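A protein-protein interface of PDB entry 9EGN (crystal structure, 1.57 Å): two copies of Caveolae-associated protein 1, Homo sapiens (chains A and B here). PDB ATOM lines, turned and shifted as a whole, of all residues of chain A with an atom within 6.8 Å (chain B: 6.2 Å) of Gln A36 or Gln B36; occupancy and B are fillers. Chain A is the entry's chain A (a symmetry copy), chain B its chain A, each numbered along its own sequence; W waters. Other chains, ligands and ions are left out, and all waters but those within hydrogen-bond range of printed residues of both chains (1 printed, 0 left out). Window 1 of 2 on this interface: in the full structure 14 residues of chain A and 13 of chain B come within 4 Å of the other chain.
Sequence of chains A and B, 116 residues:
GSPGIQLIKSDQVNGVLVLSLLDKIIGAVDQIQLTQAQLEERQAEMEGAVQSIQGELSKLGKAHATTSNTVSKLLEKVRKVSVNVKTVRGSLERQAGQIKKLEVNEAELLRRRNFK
Among the printed residues, pairs that only touch across the chains: Gln A36 with Gln B36 (3.2 Å), Ile A32 with Ile B32 (3.4 Å), Gln A36 with Thr B35 (3.8 Å) and Gln A33 with Ile B32 (3.8 Å).
O of Gln B31 sits at hydrogen-bond distance from OG1 of Thr B35, at 3.0 Å.
O of Ile B32 lies within hydrogen-bond range of NE2 of Gln A36.
NE2 of Gln A33 is in hydrogen-bond range of OE1 of Gln B31 (3.0 Å).
Of chain B, only Ile B32, Thr B35 and Gln B36 come within 4 Å of Gln A36.
Gln B36 touches one residue of chain A.
Printed residues of chain A within 4 Å of Gln B31: Gln A33.
Printed residues of chain B within 4 Å of Ile A32: Ile B32.
Of the printed residues of chain A, Ile B32 touches Ile A32 (3.4 Å), Gln A33 (3.8 Å) and Gln A36 (3.0 Å).
Gln A33 touches Gln B31, but with the chains exchanged Gln A31 does not touch Gln B33 (11.6 Å).
Gln A33 touches Ile B32, but with the chains exchanged Ile A32 does not touch Gln B33 (7.0 Å).
Gln A36 touches Thr B35, but with the chains exchanged Thr A35 does not touch Gln B36 (7.7 Å).
Gln A36 touches its own counterpart, Gln B36.
Positions printed for both chains: 31, 32, 33, 34, 35, 36, 37, 38, 39, 40 and 41.
Of the 6 pairs that touch across the chains among the printed residues, 2 have their exchanged pair printed and touching as well.
Water W1 bridges the side-chain amide oxygen (OE1) of Gln A36 (3.0 Å) and the side-chain amide oxygen (OE1) of Gln B31 (3.3 Å).
Of the 11 printed residues of chain A, 3 touch a printed residue of chain B.
Hydrophobic or aromatic side chains of chain A that line the printed part of chain B: Ile A32.
Printed residues of chain B that touch a printed residue of chain A: Gln B31, Ile B32, Thr B35 and Gln B36.
Hydrophobic or aromatic side chains of chain B that line the printed part of chain A: Ile B32.
Along chain B the printed residues that touch a printed residue of chain A span positions 31 to 36.
Among the printed residues, 6 pairs touch across the chains.
Among the printed residues, no Asp or Glu carboxylate lies within 4 Å of a Lys or Arg side-chain nitrogen of the other chain.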
ATOM      1  N   GLN A  31       8.179   6.916   3.991  1.00  0.00           N
ATOM      2  CA  GLN A  31       7.347   8.107   3.818  1.00  0.00           C
ATOM      3  C   GLN A  31       8.179   9.373   3.850  1.00  0.00           C
ATOM      4  O   GLN A  31       8.013  10.255   3.008  1.00  0.00           O
ATOM      5  CB  GLN A  31       6.293   8.183   4.932  1.00  0.00           C
ATOM      6  CG  GLN A  31       5.560   9.521   4.976  1.00  0.00           C
ATOM      7  CD  GLN A  31       4.529   9.528   6.065  1.00  0.00           C
ATOM      8  OE1 GLN A  31       4.887   9.297   7.238  1.00  0.00           O
ATOM      9  NE2 GLN A  31       3.286   9.846   5.733  1.00  0.00           N
ATOM     10  N   ILE A  32       9.102   9.464   4.785  1.00  0.00           N
ATOM     11  CA  ILE A  32       9.895  10.663   4.923  1.00  0.00           C
ATOM     12  C   ILE A  32      10.743  10.879   3.679  1.00  0.00           C
ATOM     13  O   ILE A  32      10.899  12.002   3.195  1.00  0.00           O
ATOM     14  CB  ILE A  32      10.773  10.565   6.173  1.00  0.00           C
ATOM     15  CG1 ILE A  32       9.939  10.539   7.458  1.00  0.00           C
ATOM     16  CG2 ILE A  32      11.774  11.664   6.197  1.00  0.00           C
ATOM     17  CD1 ILE A  32      10.756   9.997   8.631  1.00  0.00           C
ATOM     18  N   GLN A  33      11.363   9.814   3.169  1.00  0.00           N
ATOM     19  CA  GLN A  33      12.227   9.977   1.996  1.00  0.00           C
ATOM     20  C   GLN A  33      11.435  10.385   0.761  1.00  0.00           C
ATOM     21  O   GLN A  33      11.906  11.205  -0.032  1.00  0.00           O
ATOM     22  CB  GLN A  33      13.054   8.714   1.768  1.00  0.00           C
ATOM     23  CG  GLN A  33      14.156   8.534   2.803  1.00  0.00           C
ATOM     24  CD  GLN A  33      15.037   7.370   2.547  1.00  0.00           C
ATOM     25  OE1 GLN A  33      14.568   6.326   2.104  1.00  0.00           O
ATOM     26  NE2 GLN A  33      16.326   7.550   2.749  1.00  0.00           N
ATOM     27  N   LEU A  34      10.247   9.815   0.567  1.00  0.00           N
ATOM     28  CA  LEU A  34       9.382  10.244  -0.527  1.00  0.00           C
ATOM     29  C   LEU A  34       8.976  11.700  -0.384  1.00  0.00           C
ATOM     30  O   LEU A  34       9.053  12.463  -1.361  1.00  0.00           O
ATOM     31  CB  LEU A  34       8.141   9.360  -0.552  1.00  0.00           C
ATOM     32  CG  LEU A  34       8.317   7.900  -0.973  1.00  0.00           C
ATOM     33  CD1 LEU A  34       7.026   7.150  -0.702  1.00  0.00           C
ATOM     34  CD2 LEU A  34       8.683   7.766  -2.415  1.00  0.00           C
ATOM     35  N   THR A  35       8.624  12.114   0.836  1.00  0.00           N
ATOM     36  CA  THR A  35       8.218  13.494   1.081  1.00  0.00           C
ATOM     37  C   THR A  35       9.377  14.449   0.859  1.00  0.00           C
ATOM     38  O   THR A  35       9.178  15.548   0.344  1.00  0.00           O
ATOM     39  CB  THR A  35       7.610  13.610   2.480  1.00  0.00           C
ATOM     40  OG1 THR A  35       6.449  12.727   2.549  1.00  0.00           O
ATOM     41  CG2 THR A  35       7.164  15.008   2.800  1.00  0.00           C
ATOM     42  N   GLN A  36      10.608  14.077   1.277  1.00  0.00           N
ATOM     43  CA  GLN A  36      11.765  14.936   1.075  1.00  0.00           C
ATOM     44  C   GLN A  36      12.049  15.198  -0.392  1.00  0.00           C
ATOM     45  O   GLN A  36      12.446  16.308  -0.780  1.00  0.00           O
ATOM     46  CB  GLN A  36      13.010  14.326   1.694  1.00  0.00           C
ATOM     47  CG  GLN A  36      13.054  14.577   3.096  1.00  0.00           C
ATOM     48  CD  GLN A  36      14.405  14.240   3.719  1.00  0.00           C
ATOM     49  OE1 GLN A  36      15.160  13.386   3.253  1.00  0.00           O
ATOM     50  NE2 GLN A  36      14.766  15.035   4.697  1.00  0.00           N
ATOM     51  N   ALA A  37      11.888  14.201  -1.220  1.00  0.00           N
ATOM     52  CA  ALA A  37      12.086  14.416  -2.640  1.00  0.00           C
ATOM     53  C   ALA A  37      11.040  15.370  -3.203  1.00  0.00           C
ATOM     54  O   ALA A  37      11.371  16.229  -4.021  1.00  0.00           O
ATOM     55  CB  ALA A  37      12.102  13.089  -3.363  1.00  0.00           C
ATOM     56  N   GLN A  38       9.804  15.293  -2.712  1.00  0.00           N
ATOM     57  CA  GLN A  38       8.762  16.207  -3.183  1.00  0.00           C
ATOM     58  C   GLN A  38       8.963  17.632  -2.707  1.00  0.00           C
ATOM     59  O   GLN A  38       8.750  18.576  -3.480  1.00  0.00           O
ATOM     60  CB  GLN A  38       7.403  15.686  -2.711  1.00  0.00           C
ATOM     61  CG  GLN A  38       6.935  14.529  -3.504  1.00  0.00           C
ATOM     62  CD  GLN A  38       5.848  13.740  -2.820  1.00  0.00           C
ATOM     63  OE1 GLN A  38       5.409  12.700  -3.319  1.00  0.00           O
ATOM     64  NE2 GLN A  38       5.343  14.267  -1.721  1.00  0.00           N
ATOM     65  N   LEU A  39       9.367  17.815  -1.454  1.00  0.00           N
ATOM     66  CA  LEU A  39       9.671  19.156  -0.939  1.00  0.00           C
ATOM     67  C   LEU A  39      10.851  19.759  -1.718  1.00  0.00           C
ATOM     68  O   LEU A  39      10.821  20.946  -2.069  1.00  0.00           O
ATOM     69  CB  LEU A  39       9.967  19.107   0.580  1.00  0.00           C
ATOM     70  CG  LEU A  39       8.953  18.585   1.650  1.00  0.00           C
ATOM     71  CD1 LEU A  39       9.525  18.501   3.105  1.00  0.00           C
ATOM     72  CD2 LEU A  39       7.644  19.335   1.658  1.00  0.00           C
ATOM     73  N   GLU A  40      11.876  18.951  -2.065  1.00  0.00           N
ATOM     74  CA  GLU A  40      12.962  19.452  -2.913  1.00  0.00           C
ATOM     75  C   GLU A  40      12.468  19.892  -4.287  1.00  0.00           C
ATOM     76  O   GLU A  40      12.859  20.954  -4.784  1.00  0.00           O
ATOM     77  CB  GLU A  40      14.058  18.400  -3.104  1.00  0.00           C
ATOM     78  CG  GLU A  40      15.077  18.933  -4.121  1.00  0.00           C
ATOM     79  CD  GLU A  40      16.262  18.061  -4.346  1.00  0.00           C
ATOM     80  OE1 GLU A  40      16.627  17.263  -3.454  1.00  0.00           O
ATOM     81  OE2 GLU A  40      16.855  18.238  -5.425  1.00  0.00           O
ATOM     82  N   GLU A  41      11.649  19.088  -4.936  1.00  0.00           N
ATOM     83  CA  GLU A  41      11.120  19.469  -6.243  1.00  0.00           C
ATOM     84  C   GLU A  41      10.329  20.764  -6.181  1.00  0.00           C
ATOM     85  O   GLU A  41      10.488  21.627  -7.049  1.00  0.00           O
ATOM     86  CB  GLU A  41      10.302  18.320  -6.841  1.00  0.00           C
ATOM     87  CG  GLU A  41       9.611  18.681  -8.181  1.00  0.00           C
ATOM     88  CD  GLU A  41       9.312  17.484  -9.082  1.00  0.00           C
ATOM     89  OE1 GLU A  41       8.622  16.577  -8.598  1.00  0.00           O
ATOM     90  OE2 GLU A  41       9.723  17.455 -10.281  1.00  0.00           O
ATOM     91  N   GLN B  31      20.907  10.395   6.512  1.00  0.00           N
ATOM     92  CA  GLN B  31      20.700  11.114   5.254  1.00  0.00           C
ATOM     93  C   GLN B  31      19.538  12.080   5.353  1.00  0.00           C
ATOM     94  O   GLN B  31      19.642  13.233   4.934  1.00  0.00           O
ATOM     95  CB  GLN B  31      20.420  10.121   4.116  1.00  0.00           C
ATOM     96  CG  GLN B  31      19.938  10.795   2.835  1.00  0.00           C
ATOM     97  CD  GLN B  31      19.705   9.782   1.755  1.00  0.00           C
ATOM     98  OE1 GLN B  31      18.908   8.846   1.967  1.00  0.00           O
ATOM     99  NE2 GLN B  31      20.313   9.970   0.593  1.00  0.00           N
ATOM    100  N   ILE B  32      18.441  11.646   5.937  1.00  0.00           N
ATOM    101  CA  ILE B  32      17.266  12.482   6.016  1.00  0.00           C
ATOM    102  C   ILE B  32      17.554  13.715   6.858  1.00  0.00           C
ATOM    103  O   ILE B  32      17.130  14.827   6.536  1.00  0.00           O
ATOM    104  CB  ILE B  32      16.097  11.684   6.596  1.00  0.00           C
ATOM    105  CG1 ILE B  32      15.662  10.547   5.668  1.00  0.00           C
ATOM    106  CG2 ILE B  32      14.959  12.585   6.922  1.00  0.00           C
ATOM    107  CD1 ILE B  32      14.835   9.506   6.423  1.00  0.00           C
ATOM    108  N   GLN B  33      18.231  13.535   7.994  1.00  0.00           N
ATOM    109  CA  GLN B  33      18.498  14.685   8.863  1.00  0.00           C
ATOM    110  C   GLN B  33      19.433  15.690   8.205  1.00  0.00           C
ATOM    111  O   GLN B  33      19.244  16.901   8.353  1.00  0.00           O
ATOM    112  CB  GLN B  33      19.011  14.214  10.221  1.00  0.00           C
ATOM    113  CG  GLN B  33      17.925  13.569  11.072  1.00  0.00           C
ATOM    114  CD  GLN B  33      18.373  13.193  12.434  1.00  0.00           C
ATOM    115  OE1 GLN B  33      19.503  12.748  12.613  1.00  0.00           O
ATOM    116  NE2 GLN B  33      17.531  13.432  13.418  1.00  0.00           N
ATOM    117  N   LEU B  34      20.455  15.216   7.492  1.00  0.00           N
ATOM    118  CA  LEU B  34      21.319  16.115   6.736  1.00  0.00           C
ATOM    119  C   LEU B  34      20.551  16.861   5.661  1.00  0.00           C
ATOM    120  O   LEU B  34      20.700  18.087   5.531  1.00  0.00           O
ATOM    121  CB  LEU B  34      22.442  15.302   6.101  1.00  0.00           C
ATOM    122  CG  LEU B  34      23.504  14.710   7.029  1.00  0.00           C
ATOM    123  CD1 LEU B  34      24.376  13.756   6.234  1.00  0.00           C
ATOM    124  CD2 LEU B  34      24.355  15.762   7.662  1.00  0.00           C
ATOM    125  N   THR B  35      19.670  16.156   4.945  1.00  0.00           N
ATOM    126  CA  THR B  35      18.880  16.778   3.888  1.00  0.00           C
ATOM    127  C   THR B  35      17.915  17.800   4.462  1.00  0.00           C
ATOM    128  O   THR B  35      17.691  18.845   3.852  1.00  0.00           O
ATOM    129  CB  THR B  35      18.180  15.696   3.064  1.00  0.00           C
ATOM    130  OG1 THR B  35      19.204  14.832   2.480  1.00  0.00           O
ATOM    131  CG2 THR B  35      17.349  16.267   1.951  1.00  0.00           C
ATOM    132  N   GLN B  36      17.288  17.513   5.624  1.00  0.00           N
ATOM    133  CA  GLN B  36      16.368  18.458   6.239  1.00  0.00           C
ATOM    134  C   GLN B  36      17.038  19.765   6.614  1.00  0.00           C
ATOM    135  O   GLN B  36      16.447  20.849   6.489  1.00  0.00           O
ATOM    136  CB  GLN B  36      15.742  17.872   7.493  1.00  0.00           C
ATOM    137  CG  GLN B  36      14.657  17.011   7.163  1.00  0.00           C
ATOM    138  CD  GLN B  36      13.817  16.620   8.376  1.00  0.00           C
ATOM    139  OE1 GLN B  36      14.278  16.572   9.517  1.00  0.00           O
ATOM    140  NE2 GLN B  36      12.535  16.488   8.130  1.00  0.00           N
ATOM    141  N   ALA B  37      18.249  19.699   7.102  1.00  0.00           N
ATOM    142  CA  ALA B  37      18.956  20.923   7.418  1.00  0.00           C
ATOM    143  C   ALA B  37      19.247  21.733   6.161  1.00  0.00           C
ATOM    144  O   ALA B  37      19.116  22.956   6.175  1.00  0.00           O
ATOM    145  CB  ALA B  37      20.211  20.604   8.199  1.00  0.00           C
ATOM    146  N   GLN B  38      19.549  21.061   5.051  1.00  0.00           N
ATOM    147  CA  GLN B  38      19.801  21.777   3.798  1.00  0.00           C
ATOM    148  C   GLN B  38      18.549  22.386   3.200  1.00  0.00           C
ATOM    149  O   GLN B  38      18.592  23.518   2.699  1.00  0.00           O
ATOM    150  CB  GLN B  38      20.438  20.808   2.800  1.00  0.00           C
ATOM    151  CG  GLN B  38      21.863  20.548   3.094  1.00  0.00           C
ATOM    152  CD  GLN B  38      22.394  19.308   2.422  1.00  0.00           C
ATOM    153  OE1 GLN B  38      23.544  18.914   2.632  1.00  0.00           O
ATOM    154  NE2 GLN B  38      21.598  18.733   1.540  1.00  0.00           N
ATOM    155  N   LEU B  39      17.432  21.667   3.238  1.00  0.00           N
ATOM    156  CA  LEU B  39      16.155  22.215   2.763  1.00  0.00           C
ATOM    157  C   LEU B  39      15.754  23.425   3.622  1.00  0.00           C
ATOM    158  O   LEU B  39      15.292  24.440   3.086  1.00  0.00           O
ATOM    159  CB  LEU B  39      15.052  21.129   2.773  1.00  0.00           C
ATOM    160  CG  LEU B  39      15.137  19.791   1.966  1.00  0.00           C
ATOM    161  CD1 LEU B  39      13.968  18.787   2.242  1.00  0.00           C
ATOM    162  CD2 LEU B  39      15.299  19.993   0.479  1.00  0.00           C
ATOM    163  N   GLU B  40      15.983  23.376   4.952  1.00  0.00           N
ATOM    164  CA  GLU B  40      15.730  24.550   5.793  1.00  0.00           C
ATOM    165  C   GLU B  40      16.598  25.741   5.398  1.00  0.00           C
ATOM    166  O   GLU B  40      16.110  26.872   5.309  1.00  0.00           O
ATOM    167  CB  GLU B  40      15.969  24.245   7.273  1.00  0.00           C
ATOM    168  CG  GLU B  40      15.840  25.550   8.071  1.00  0.00           C
ATOM    169  CD  GLU B  40      15.951  25.404   9.548  1.00  0.00           C
ATOM    170  OE1 GLU B  40      15.672  24.312  10.089  1.00  0.00           O
ATOM    171  OE2 GLU B  40      16.275  26.437  10.161  1.00  0.00           O
ATOM    172  N   GLU B  41      17.884  25.528   5.197  1.00  0.00           N
ATOM    173  CA  GLU B  41      18.760  26.624   4.789  1.00  0.00           C
ATOM    174  C   GLU B  41      18.319  27.246   3.475  1.00  0.00           C
ATOM    175  O   GLU B  41      18.299  28.474   3.349  1.00  0.00           O
ATOM    176  CB  GLU B  41      20.216  26.153   4.746  1.00  0.00           C
ATOM    177  CG  GLU B  41      21.201  27.225   4.214  1.00  0.00           C
ATOM    178  CD  GLU B  41      22.642  27.054   4.693  1.00  0.00           C
ATOM    179  OE1 GLU B  41      23.188  25.970   4.451  1.00  0.00           O
ATOM    180  OE2 GLU B  41      23.252  28.005   5.271  1.00  0.00           O
HETATM  181  O   HOH W   1      16.399  11.018   1.925  1.00  0.00           O
